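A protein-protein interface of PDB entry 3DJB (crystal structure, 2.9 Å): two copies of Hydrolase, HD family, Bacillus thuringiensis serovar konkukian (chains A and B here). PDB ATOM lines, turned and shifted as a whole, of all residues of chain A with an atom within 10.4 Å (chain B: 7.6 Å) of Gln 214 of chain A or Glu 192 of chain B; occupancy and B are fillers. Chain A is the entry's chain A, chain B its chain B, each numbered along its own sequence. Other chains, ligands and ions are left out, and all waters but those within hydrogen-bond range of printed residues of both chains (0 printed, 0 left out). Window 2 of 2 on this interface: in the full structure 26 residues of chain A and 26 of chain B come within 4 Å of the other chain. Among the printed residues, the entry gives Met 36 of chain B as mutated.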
ATOM      1  N   ILE A 204      -0.204 -23.887  15.952  1.00  0.00           N
ATOM      2  CA  ILE A 204      -1.130 -24.832  16.572  1.00  0.00           C
ATOM      3  C   ILE A 204      -0.647 -25.158  17.989  1.00  0.00           C
ATOM      4  O   ILE A 204      -1.389 -25.716  18.804  1.00  0.00           O
ATOM      5  CB  ILE A 204      -1.267 -26.135  15.720  1.00  0.00           C
ATOM      6  CG1 ILE A 204      -1.793 -25.790  14.319  1.00  0.00           C
ATOM      7  CG2 ILE A 204      -2.255 -27.096  16.362  1.00  0.00           C
ATOM      8  CD1 ILE A 204      -2.112 -27.004  13.455  1.00  0.00           C
ATOM      9  N   GLU A 205       0.593 -24.781  18.286  1.00  0.00           N
ATOM     10  CA  GLU A 205       1.158 -25.012  19.605  1.00  0.00           C
ATOM     11  C   GLU A 205       0.775 -23.854  20.504  1.00  0.00           C
ATOM     12  O   GLU A 205       0.540 -24.036  21.695  1.00  0.00           O
ATOM     13  CB  GLU A 205       2.672 -25.106  19.525  1.00  0.00           C
ATOM     14  CG  GLU A 205       3.306 -25.798  20.710  1.00  0.00           C
ATOM     15  CD  GLU A 205       4.648 -26.404  20.354  1.00  0.00           C
ATOM     16  OE1 GLU A 205       5.553 -25.616  19.966  1.00  0.00           O
ATOM     17  OE2 GLU A 205       4.791 -27.658  20.456  1.00  0.00           O
ATOM     18  N   GLN A 206       0.723 -22.657  19.935  1.00  0.00           N
ATOM     19  CA  GLN A 206       0.349 -21.495  20.713  1.00  0.00           C
ATOM     20  C   GLN A 206      -1.154 -21.460  20.767  1.00  0.00           C
ATOM     21  O   GLN A 206      -1.733 -20.966  21.717  1.00  0.00           O
ATOM     22  CB  GLN A 206       0.840 -20.217  20.059  1.00  0.00           C
ATOM     23  CG  GLN A 206       0.216 -18.964  20.641  1.00  0.00           C
ATOM     24  CD  GLN A 206       0.818 -18.588  21.972  1.00  0.00           C
ATOM     25  OE1 GLN A 206       0.203 -17.871  22.770  1.00  0.00           O
ATOM     26  NE2 GLN A 206       2.040 -19.057  22.216  1.00  0.00           N
ATOM     27  N   PHE A 207      -1.794 -21.980  19.732  1.00  0.00           N
ATOM     28  CA  PHE A 207      -3.243 -21.981  19.700  1.00  0.00           C
ATOM     29  C   PHE A 207      -3.797 -22.870  20.778  1.00  0.00           C
ATOM     30  O   PHE A 207      -4.740 -22.498  21.458  1.00  0.00           O
ATOM     31  CB  PHE A 207      -3.744 -22.458  18.337  1.00  0.00           C
ATOM     32  CG  PHE A 207      -5.244 -22.621  18.245  1.00  0.00           C
ATOM     33  CD1 PHE A 207      -5.883 -23.726  18.793  1.00  0.00           C
ATOM     34  CD2 PHE A 207      -6.009 -21.695  17.543  1.00  0.00           C
ATOM     35  CE1 PHE A 207      -7.260 -23.902  18.633  1.00  0.00           C
ATOM     36  CE2 PHE A 207      -7.382 -21.869  17.384  1.00  0.00           C
ATOM     37  CZ  PHE A 207      -8.004 -22.971  17.925  1.00  0.00           C
ATOM     38  N   MET A 208      -3.203 -24.046  20.940  1.00  0.00           N
ATOM     39  CA  MET A 208      -3.680 -25.013  21.926  1.00  0.00           C
ATOM     40  C   MET A 208      -3.555 -24.570  23.374  1.00  0.00           C
ATOM     41  O   MET A 208      -4.504 -24.687  24.151  1.00  0.00           O
ATOM     42  CB  MET A 208      -2.950 -26.338  21.734  1.00  0.00           C
ATOM     43  CG  MET A 208      -3.893 -27.528  21.695  1.00  0.00           C
ATOM     44  SD  MET A 208      -5.410 -27.198  20.523  1.00  0.00           S
ATOM     45  CE  MET A 208      -4.445 -27.039  18.850  1.00  0.00           C
ATOM     46  N   LYS A 209      -2.370 -24.085  23.731  1.00  0.00           N
ATOM     47  CA  LYS A 209      -2.132 -23.616  25.078  1.00  0.00           C
ATOM     48  C   LYS A 209      -3.207 -22.587  25.422  1.00  0.00           C
ATOM     49  O   LYS A 209      -3.723 -22.563  26.537  1.00  0.00           O
ATOM     50  CB  LYS A 209      -0.736 -22.996  25.192  1.00  0.00           C
ATOM     51  CG  LYS A 209      -0.492 -21.838  24.247  1.00  0.00           C
ATOM     52  CD  LYS A 209       0.685 -20.967  24.695  1.00  0.00           C
ATOM     53  CE  LYS A 209       2.031 -21.685  24.608  1.00  0.00           C
ATOM     54  NZ  LYS A 209       3.145 -20.745  24.943  1.00  0.00           N
ATOM     55  N   GLU A 210      -3.558 -21.742  24.460  1.00  0.00           N
ATOM     56  CA  GLU A 210      -4.582 -20.736  24.701  1.00  0.00           C
ATOM     57  C   GLU A 210      -5.923 -21.419  24.905  1.00  0.00           C
ATOM     58  O   GLU A 210      -6.699 -21.028  25.772  1.00  0.00           O
ATOM     59  CB  GLU A 210      -4.660 -19.749  23.529  1.00  0.00           C
ATOM     60  CG  GLU A 210      -3.587 -18.662  23.585  1.00  0.00           C
ATOM     61  CD  GLU A 210      -3.357 -17.975  22.246  1.00  0.00           C
ATOM     62  OE1 GLU A 210      -4.346 -17.536  21.612  1.00  0.00           O
ATOM     63  OE2 GLU A 210      -2.178 -17.866  21.834  1.00  0.00           O
ATOM     64  N   TRP A 211      -6.183 -22.456  24.119  1.00  0.00           N
ATOM     65  CA  TRP A 211      -7.445 -23.183  24.217  1.00  0.00           C
ATOM     66  C   TRP A 211      -7.695 -23.697  25.632  1.00  0.00           C
ATOM     67  O   TRP A 211      -8.844 -23.859  26.054  1.00  0.00           O
ATOM     68  CB  TRP A 211      -7.447 -24.353  23.233  1.00  0.00           C
ATOM     69  CG  TRP A 211      -8.726 -25.111  23.222  1.00  0.00           C
ATOM     70  CD1 TRP A 211      -9.012 -26.237  23.922  1.00  0.00           C
ATOM     71  CD2 TRP A 211      -9.906 -24.783  22.481  1.00  0.00           C
ATOM     72  NE1 TRP A 211     -10.301 -26.637  23.663  1.00  0.00           N
ATOM     73  CE2 TRP A 211     -10.871 -25.760  22.780  1.00  0.00           C
ATOM     74  CE3 TRP A 211     -10.238 -23.755  21.592  1.00  0.00           C
ATOM     75  CZ2 TRP A 211     -12.145 -25.747  22.224  1.00  0.00           C
ATOM     76  CZ3 TRP A 211     -11.508 -23.738  21.038  1.00  0.00           C
ATOM     77  CH2 TRP A 211     -12.447 -24.731  21.357  1.00  0.00           C
ATOM     78  N   ASN A 212      -6.603 -23.943  26.352  1.00  0.00           N
ATOM     79  CA  ASN A 212      -6.658 -24.435  27.720  1.00  0.00           C
ATOM     80  C   ASN A 212      -6.148 -23.363  28.667  1.00  0.00           C
ATOM     81  O   ASN A 212      -5.672 -23.660  29.763  1.00  0.00           O
ATOM     82  CB  ASN A 212      -5.783 -25.673  27.853  1.00  0.00           C
ATOM     83  CG  ASN A 212      -5.927 -26.599  26.675  1.00  0.00           C
ATOM     84  OD1 ASN A 212      -7.035 -27.037  26.358  1.00  0.00           O
ATOM     85  ND2 ASN A 212      -4.810 -26.900  26.009  1.00  0.00           N
ATOM     86  N   ALA A 213      -6.233 -22.115  28.234  1.00  0.00           N
ATOM     87  CA  ALA A 213      -5.780 -21.008  29.059  1.00  0.00           C
ATOM     88  C   ALA A 213      -4.458 -21.336  29.742  1.00  0.00           C
ATOM     89  O   ALA A 213      -4.437 -21.618  30.935  1.00  0.00           O
ATOM     90  CB  ALA A 213      -6.835 -20.684  30.111  1.00  0.00           C
ATOM     91  N   GLN A 214      -3.360 -21.305  28.989  1.00  0.00           N
ATOM     92  CA  GLN A 214      -2.060 -21.595  29.570  1.00  0.00           C
ATOM     93  C   GLN A 214      -1.408 -20.270  29.928  1.00  0.00           C
ATOM     94  O   GLN A 214      -1.427 -19.895  31.133  1.00  0.00           O
ATOM     95  CB  GLN A 214      -1.181 -22.366  28.575  1.00  0.00           C
ATOM     96  CG  GLN A 214      -0.483 -23.615  29.154  1.00  0.00           C
ATOM     97  CD  GLN A 214      -1.106 -24.947  28.695  1.00  0.00           C
ATOM     98  OE1 GLN A 214      -0.908 -25.334  27.526  1.00  0.00           O
ATOM     99  NE2 GLN A 214      -1.799 -25.606  29.501  1.00  0.00           N
ATOM    100  N   ARG B  32     -12.556 -20.995  28.982  1.00  0.00           N
ATOM    101  CA  ARG B  32     -11.261 -20.396  28.693  1.00  0.00           C
ATOM    102  C   ARG B  32     -11.035 -19.120  29.505  1.00  0.00           C
ATOM    103  O   ARG B  32      -9.929 -18.852  29.956  1.00  0.00           O
ATOM    104  CB  ARG B  32     -11.178 -20.079  27.208  1.00  0.00           C
ATOM    105  CG  ARG B  32      -9.924 -20.535  26.574  1.00  0.00           C
ATOM    106  CD  ARG B  32      -9.856 -19.981  25.181  1.00  0.00           C
ATOM    107  NE  ARG B  32     -10.855 -20.562  24.297  1.00  0.00           N
ATOM    108  CZ  ARG B  32     -11.977 -19.964  23.910  1.00  0.00           C
ATOM    109  NH1 ARG B  32     -12.811 -20.602  23.093  1.00  0.00           N
ATOM    110  NH2 ARG B  32     -12.269 -18.742  24.326  1.00  0.00           N
ATOM    111  N   LYS B  35     -11.104 -20.442  33.532  1.00  0.00           N
ATOM    112  CA  LYS B  35      -9.834 -21.040  33.918  1.00  0.00           C
ATOM    113  C   LYS B  35      -8.751 -19.963  33.942  1.00  0.00           C
ATOM    114  O   LYS B  35      -7.808 -20.017  34.727  1.00  0.00           O
ATOM    115  CB  LYS B  35      -9.455 -22.151  32.941  1.00  0.00           C
ATOM    116  CG  LYS B  35     -10.462 -23.278  32.873  1.00  0.00           C
ATOM    117  CD  LYS B  35     -10.005 -24.349  31.893  1.00  0.00           C
ATOM    118  CE  LYS B  35      -8.905 -25.235  32.460  1.00  0.00           C
ATOM    119  NZ  LYS B  35      -9.463 -26.450  33.128  1.00  0.00           N
ATOM    120  N   MET B  36      -8.910 -18.975  33.076  1.00  0.00           N
ATOM    121  CA  MET B  36      -7.965 -17.872  32.972  1.00  0.00           C
ATOM    122  C   MET B  36      -8.086 -16.889  34.152  1.00  0.00           C
ATOM    123  O   MET B  36      -7.088 -16.314  34.603  1.00  0.00           O
ATOM    124  CB  MET B  36      -8.200 -17.153  31.638  1.00  0.00           C
ATOM    125  CG  MET B  36      -7.093 -16.215  31.193  1.00  0.00           C
ATOM    126  SD  MET B  36      -6.813 -16.260  29.266  1.00  0.00           S
ATOM    127  CE  MET B  36      -8.639 -16.553  28.623  1.00  0.00           C
ATOM    128  N   SER B  39      -6.116 -18.709  37.194  1.00  0.00           N
ATOM    129  CA  SER B  39      -4.689 -18.493  37.079  1.00  0.00           C
ATOM    130  C   SER B  39      -4.264 -17.058  37.314  1.00  0.00           C
ATOM    131  O   SER B  39      -3.162 -16.796  37.806  1.00  0.00           O
ATOM    132  CB  SER B  39      -4.208 -18.967  35.715  1.00  0.00           C
ATOM    133  OG  SER B  39      -4.478 -20.346  35.578  1.00  0.00           O
ATOM    134  N   LEU B  40      -5.148 -16.130  36.977  1.00  0.00           N
ATOM    135  CA  LEU B  40      -4.867 -14.709  37.150  1.00  0.00           C
ATOM    136  C   LEU B  40      -4.958 -14.306  38.637  1.00  0.00           C
ATOM    137  O   LEU B  40      -4.068 -13.624  39.162  1.00  0.00           O
ATOM    138  CB  LEU B  40      -5.847 -13.894  36.293  1.00  0.00           C
ATOM    139  CG  LEU B  40      -5.327 -12.785  35.374  1.00  0.00           C
ATOM    140  CD1 LEU B  40      -4.203 -13.281  34.477  1.00  0.00           C
ATOM    141  CD2 LEU B  40      -6.487 -12.276  34.545  1.00  0.00           C
ATOM    142  N   ASP B 120      -9.958  -8.762  32.992  1.00  0.00           N
ATOM    143  CA  ASP B 120      -8.670  -8.987  32.362  1.00  0.00           C
ATOM    144  C   ASP B 120      -8.656 -10.381  31.774  1.00  0.00           C
ATOM    145  O   ASP B 120      -7.914 -10.670  30.831  1.00  0.00           O
ATOM    146  CB  ASP B 120      -7.551  -8.863  33.382  1.00  0.00           C
ATOM    147  CG  ASP B 120      -7.233  -7.428  33.712  1.00  0.00           C
ATOM    148  OD1 ASP B 120      -6.578  -7.206  34.752  1.00  0.00           O
ATOM    149  OD2 ASP B 120      -7.628  -6.530  32.927  1.00  0.00           O
ATOM    150  N   LEU B 124      -8.479 -10.684  27.498  1.00  0.00           N
ATOM    151  CA  LEU B 124      -7.323 -11.456  27.045  1.00  0.00           C
ATOM    152  C   LEU B 124      -7.764 -12.481  26.024  1.00  0.00           C
ATOM    153  O   LEU B 124      -6.999 -12.845  25.129  1.00  0.00           O
ATOM    154  CB  LEU B 124      -6.674 -12.180  28.212  1.00  0.00           C
ATOM    155  CG  LEU B 124      -5.652 -11.332  28.947  1.00  0.00           C
ATOM    156  CD1 LEU B 124      -5.270 -11.992  30.270  1.00  0.00           C
ATOM    157  CD2 LEU B 124      -4.452 -11.151  28.052  1.00  0.00           C
ATOM    158  N   LEU B 127      -7.100 -11.866  22.018  1.00  0.00           N
ATOM    159  CA  LEU B 127      -5.770 -11.818  21.448  1.00  0.00           C
ATOM    160  C   LEU B 127      -5.148 -13.211  21.375  1.00  0.00           C
ATOM    161  O   LEU B 127      -5.590 -14.147  22.055  1.00  0.00           O
ATOM    162  CB  LEU B 127      -4.874 -10.905  22.295  1.00  0.00           C
ATOM    163  CG  LEU B 127      -5.522  -9.757  23.076  1.00  0.00           C
ATOM    164  CD1 LEU B 127      -4.482  -8.990  23.901  1.00  0.00           C
ATOM    165  CD2 LEU B 127      -6.192  -8.841  22.104  1.00  0.00           C
ATOM    166  N   LYS B 181      -3.984  -4.811  24.579  1.00  0.00           N
ATOM    167  CA  LYS B 181      -3.001  -5.108  25.611  1.00  0.00           C
ATOM    168  C   LYS B 181      -2.712  -3.881  26.457  1.00  0.00           C
ATOM    169  O   LYS B 181      -1.965  -3.945  27.429  1.00  0.00           O
ATOM    170  CB  LYS B 181      -1.708  -5.629  24.966  1.00  0.00           C
ATOM    171  CG  LYS B 181      -1.171  -4.771  23.823  1.00  0.00           C
ATOM    172  CD  LYS B 181      -0.219  -3.674  24.279  1.00  0.00           C
ATOM    173  CE  LYS B 181       1.159  -4.219  24.615  1.00  0.00           C
ATOM    174  NZ  LYS B 181       1.123  -5.155  25.771  1.00  0.00           N
ATOM    175  N   MET B 184      -5.418  -3.757  29.779  1.00  0.00           N
ATOM    176  CA  MET B 184      -5.335  -4.777  30.810  1.00  0.00           C
ATOM    177  C   MET B 184      -5.130  -4.077  32.155  1.00  0.00           C
ATOM    178  O   MET B 184      -4.414  -3.079  32.231  1.00  0.00           O
ATOM    179  CB  MET B 184      -4.172  -5.722  30.492  1.00  0.00           C
ATOM    180  CG  MET B 184      -4.530  -7.220  30.529  1.00  0.00           C
ATOM    181  SD  MET B 184      -5.978  -7.775  29.323  1.00  0.00           S
ATOM    182  CE  MET B 184      -5.020  -7.958  27.672  1.00  0.00           C
ATOM    183  N   THR B 186      -4.711  -5.782  35.957  1.00  0.00           N
ATOM    184  CA  THR B 186      -3.677  -6.376  36.813  1.00  0.00           C
ATOM    185  C   THR B 186      -2.412  -6.700  36.036  1.00  0.00           C
ATOM    186  O   THR B 186      -2.380  -6.649  34.808  1.00  0.00           O
ATOM    187  CB  THR B 186      -4.104  -7.700  37.489  1.00  0.00           C
ATOM    188  OG1 THR B 186      -3.812  -8.783  36.606  1.00  0.00           O
ATOM    189  CG2 THR B 186      -5.578  -7.716  37.820  1.00  0.00           C
ATOM    190  N   ASN B 187      -1.371  -7.067  36.774  1.00  0.00           N
ATOM    191  CA  ASN B 187      -0.090  -7.405  36.175  1.00  0.00           C
ATOM    192  C   ASN B 187      -0.132  -8.705  35.384  1.00  0.00           C
ATOM    193  O   ASN B 187       0.176  -8.702  34.203  1.00  0.00           O
ATOM    194  CB  ASN B 187       0.994  -7.511  37.257  1.00  0.00           C
ATOM    195  CG  ASN B 187       1.358  -6.168  37.870  1.00  0.00           C
ATOM    196  OD1 ASN B 187       2.175  -6.103  38.791  1.00  0.00           O
ATOM    197  ND2 ASN B 187       0.764  -5.092  37.361  1.00  0.00           N
ATOM    198  N   ALA B 188      -0.500  -9.810  36.036  1.00  0.00           N
ATOM    199  CA  ALA B 188      -0.549 -11.115  35.373  1.00  0.00           C
ATOM    200  C   ALA B 188      -1.230 -11.034  34.004  1.00  0.00           C
ATOM    201  O   ALA B 188      -0.761 -11.632  33.020  1.00  0.00           O
ATOM    202  CB  ALA B 188      -1.261 -12.136  36.257  1.00  0.00           C
ATOM    203  N   ALA B 189      -2.333 -10.288  33.954  1.00  0.00           N
ATOM    204  CA  ALA B 189      -3.096 -10.079  32.722  1.00  0.00           C
ATOM    205  C   ALA B 189      -2.228  -9.306  31.743  1.00  0.00           C
ATOM    206  O   ALA B 189      -2.126  -9.670  30.578  1.00  0.00           O
ATOM    207  CB  ALA B 189      -4.366  -9.296  33.016  1.00  0.00           C
ATOM    208  N   LYS B 190      -1.610  -8.231  32.218  1.00  0.00           N
ATOM    209  CA  LYS B 190      -0.743  -7.447  31.357  1.00  0.00           C
ATOM    210  C   LYS B 190       0.386  -8.313  30.817  1.00  0.00           C
ATOM    211  O   LYS B 190       0.720  -8.246  29.642  1.00  0.00           O
ATOM    212  CB  LYS B 190      -0.155  -6.243  32.106  1.00  0.00           C
ATOM    213  CG  LYS B 190      -1.109  -5.061  32.276  1.00  0.00           C
ATOM    214  CD  LYS B 190      -0.356  -3.744  32.505  1.00  0.00           C
ATOM    215  CE  LYS B 190       0.793  -3.529  31.485  1.00  0.00           C
ATOM    216  NZ  LYS B 190       0.418  -3.464  30.027  1.00  0.00           N
ATOM    217  N   GLN B 191       0.977  -9.131  31.678  1.00  0.00           N
ATOM    218  CA  GLN B 191       2.070  -9.989  31.252  1.00  0.00           C
ATOM    219  C   GLN B 191       1.620 -10.872  30.110  1.00  0.00           C
ATOM    220  O   GLN B 191       2.108 -10.757  28.986  1.00  0.00           O
ATOM    221  CB  GLN B 191       2.552 -10.865  32.404  1.00  0.00           C
ATOM    222  CG  GLN B 191       3.508 -11.968  31.966  1.00  0.00           C
ATOM    223  CD  GLN B 191       4.657 -11.465  31.080  1.00  0.00           C
ATOM    224  OE1 GLN B 191       4.472 -11.186  29.886  1.00  0.00           O
ATOM    225  NE2 GLN B 191       5.846 -11.338  31.671  1.00  0.00           N
ATOM    226  N   GLU B 192       0.691 -11.765  30.408  1.00  0.00           N
ATOM    227  CA  GLU B 192       0.166 -12.658  29.395  1.00  0.00           C
ATOM    228  C   GLU B 192      -0.145 -11.884  28.112  1.00  0.00           C
ATOM    229  O   GLU B 192       0.249 -12.305  27.026  1.00  0.00           O
ATOM    230  CB  GLU B 192      -1.099 -13.330  29.924  1.00  0.00           C
ATOM    231  CG  GLU B 192      -1.839 -14.154  28.903  1.00  0.00           C
ATOM    232  CD  GLU B 192      -1.018 -15.307  28.382  1.00  0.00           C
ATOM    233  OE1 GLU B 192      -0.218 -15.088  27.455  1.00  0.00           O
ATOM    234  OE2 GLU B 192      -1.164 -16.429  28.909  1.00  0.00           O
ATOM    235  N   ALA B 193      -0.835 -10.748  28.253  1.00  0.00           N
ATOM    236  CA  ALA B 193      -1.239  -9.893  27.129  1.00  0.00           C
ATOM    237  C   ALA B 193      -0.086  -9.492  26.218  1.00  0.00           C
ATOM    238  O   ALA B 193      -0.230  -9.472  24.992  1.00  0.00           O
ATOM    239  CB  ALA B 193      -1.930  -8.654  27.650  1.00  0.00           C
ATOM    240  N   GLU B 194       1.049  -9.149  26.822  1.00  0.00           N
ATOM    241  CA  GLU B 194       2.229  -8.782  26.062  1.00  0.00           C
ATOM    242  C   GLU B 194       2.684  -9.990  25.257  1.00  0.00           C
ATOM    243  O   GLU B 194       3.040  -9.870  24.094  1.00  0.00           O
ATOM    244  CB  GLU B 194       3.348  -8.346  27.003  1.00  0.00           C
ATOM    245  CG  GLU B 194       3.569  -6.846  27.020  1.00  0.00           C
ATOM    246  CD  GLU B 194       4.102  -6.321  25.695  1.00  0.00           C
ATOM    247  OE1 GLU B 194       4.061  -5.085  25.488  1.00  0.00           O
ATOM    248  OE2 GLU B 194       4.565  -7.143  24.869  1.00  0.00           O
ATOM    249  N   VAL B 195       2.662 -11.163  25.875  1.00  0.00           N
ATOM    250  CA  VAL B 195       3.092 -12.356  25.174  1.00  0.00           C
ATOM    251  C   VAL B 195       2.111 -12.642  24.047  1.00  0.00           C
ATOM    252  O   VAL B 195       2.524 -12.926  22.919  1.00  0.00           O
ATOM    253  CB  VAL B 195       3.177 -13.575  26.117  1.00  0.00           C
ATOM    254  CG1 VAL B 195       4.167 -14.562  25.574  1.00  0.00           C
ATOM    255  CG2 VAL B 195       3.595 -13.133  27.504  1.00  0.00           C
ATOM    256  N   ARG B 196       0.814 -12.561  24.340  1.00  0.00           N
ATOM    257  CA  ARG B 196      -0.224 -12.816  23.329  1.00  0.00           C
ATOM    258  C   ARG B 196      -0.139 -11.791  22.200  1.00  0.00           C
ATOM    259  O   ARG B 196      -0.180 -12.153  21.014  1.00  0.00           O
ATOM    260  CB  ARG B 196      -1.631 -12.712  23.927  1.00  0.00           C
ATOM    261  CG  ARG B 196      -2.132 -13.895  24.748  1.00  0.00           C
ATOM    262  CD  ARG B 196      -3.542 -14.226  24.266  1.00  0.00           C
ATOM    263  NE  ARG B 196      -4.376 -14.887  25.259  1.00  0.00           N
ATOM    264  CZ  ARG B 196      -4.008 -15.944  25.970  1.00  0.00           C
ATOM    265  NH1 ARG B 196      -2.806 -16.468  25.809  1.00  0.00           N
ATOM    266  NH2 ARG B 196      -4.850 -16.490  26.831  1.00  0.00           N
ATOM    267  N   HIS B 197      -0.047 -10.515  22.591  1.00  0.00           N
ATOM    268  CA  HIS B 197       0.024  -9.397  21.649  1.00  0.00           C
ATOM    269  C   HIS B 197       1.212  -9.555  20.715  1.00  0.00           C
ATOM    270  O   HIS B 197       1.093  -9.388  19.496  1.00  0.00           O
ATOM    271  CB  HIS B 197       0.129  -8.059  22.404  1.00  0.00           C
ATOM    272  CG  HIS B 197       0.145  -6.851  21.509  1.00  0.00           C
ATOM    273  ND1 HIS B 197       1.296  -6.143  21.226  1.00  0.00           N
ATOM    274  CD2 HIS B 197      -0.853  -6.217  20.846  1.00  0.00           C
ATOM    275  CE1 HIS B 197       1.007  -5.127  20.430  1.00  0.00           C
ATOM    276  NE2 HIS B 197      -0.291  -5.149  20.184  1.00  0.00           N
ATOM    277  N   ARG B 198       2.353  -9.900  21.297  1.00  0.00           N
ATOM    278  CA  ARG B 198       3.577 -10.083  20.542  1.00  0.00           C
ATOM    279  C   ARG B 198       3.364 -11.071  19.412  1.00  0.00           C
ATOM    280  O   ARG B 198       3.804 -10.818  18.294  1.00  0.00           O
ATOM    281  CB  ARG B 198       4.674 -10.598  21.464  1.00  0.00           C
ATOM    282  CG  ARG B 198       6.086 -10.439  20.932  1.00  0.00           C
ATOM    283  CD  ARG B 198       7.078 -10.991  21.947  1.00  0.00           C
ATOM    284  NE  ARG B 198       6.726 -10.598  23.313  1.00  0.00           N
ATOM    285  CZ  ARG B 198       6.599  -9.339  23.734  1.00  0.00           C
ATOM    286  NH1 ARG B 198       6.272  -9.088  24.995  1.00  0.00           N
ATOM    287  NH2 ARG B 198       6.796  -8.323  22.903  1.00  0.00           N
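Glu 210 of chain A touches Arg 32 of chain B.
Glu 210 of chain A touches Leu 127 of chain B (OE1 to O, 3.6 Å).
Arg 196 of chain B touches Glu 210 of chain A (NH1 to CG, 3.2 Å).
Trp 211 of chain A touches Arg 32 of chain B (O to CG, 3.5 Å).
Ala 213 of chain A touches Arg 32 of chain B (CB to O, 3.6 Å).
Gln 214 of chain A touches Glu 192 of chain B.
No position is printed for both chains.
Of the 23 printed residues of chain B, 4 touch a printed residue of chain A.
Among the printed residues, 6 pairs touch across the chains.
Among the printed residues, no Asp or Glu carboxylate lies within 4 Å of a Lys or Arg side-chain nitrogen of the other chain.
The side-chain amide oxygen (OE1) of Gln 206 of chain A sits close to the side-chain carboxylate (OE2) of Glu 210 of chain A, 2.6 Å away.
O of Lys 209 of chain A is in hydrogen-bond range of N of Gln 214 of chain A.
The side-chain sulfur (SD) of Met 36 of chain B is in hydrogen-bond range of the guanidinium group (NH2) of Arg 196 of chain B, 3.1 Å away.
O of Leu 124 of chain B is in hydrogen-bond range of NE of Arg 196 of chain B (3.3 Å).
NH1 of Arg 196 of chain B is in salt-bridge range of OE1 of Glu 192 of chain B, at 3.4 Å.
Of the printed residues of chain A, Glu 192 of chain B touches Gln 214.
No residue of chain A comes within 4 Å of Ala 188 of chain B.
No residue of chain A comes within 4 Å of Ala 189 of chain B.
No residue of chain A comes within 4 Å of Ala 193 of chain B.
No residue of chain A comes within 4 Å of Val 195 of chain B.
Printed residues of chain A within 4 Å of Arg 32 of chain B: Glu 210, Trp 211 and Ala 213.
Printed residues of chain A within 4 Å of Leu 127 of chain B: Glu 210.
Of the printed residues of chain B, Ala 213 of chain A touches Arg 32 (3.6 Å).
Met 208 of chain A touches none of the printed residues of chain B.
The nearest printed residue of chain A that does not touch Leu 127 of chain B is Gln 206 of chain A (6.9 Å).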
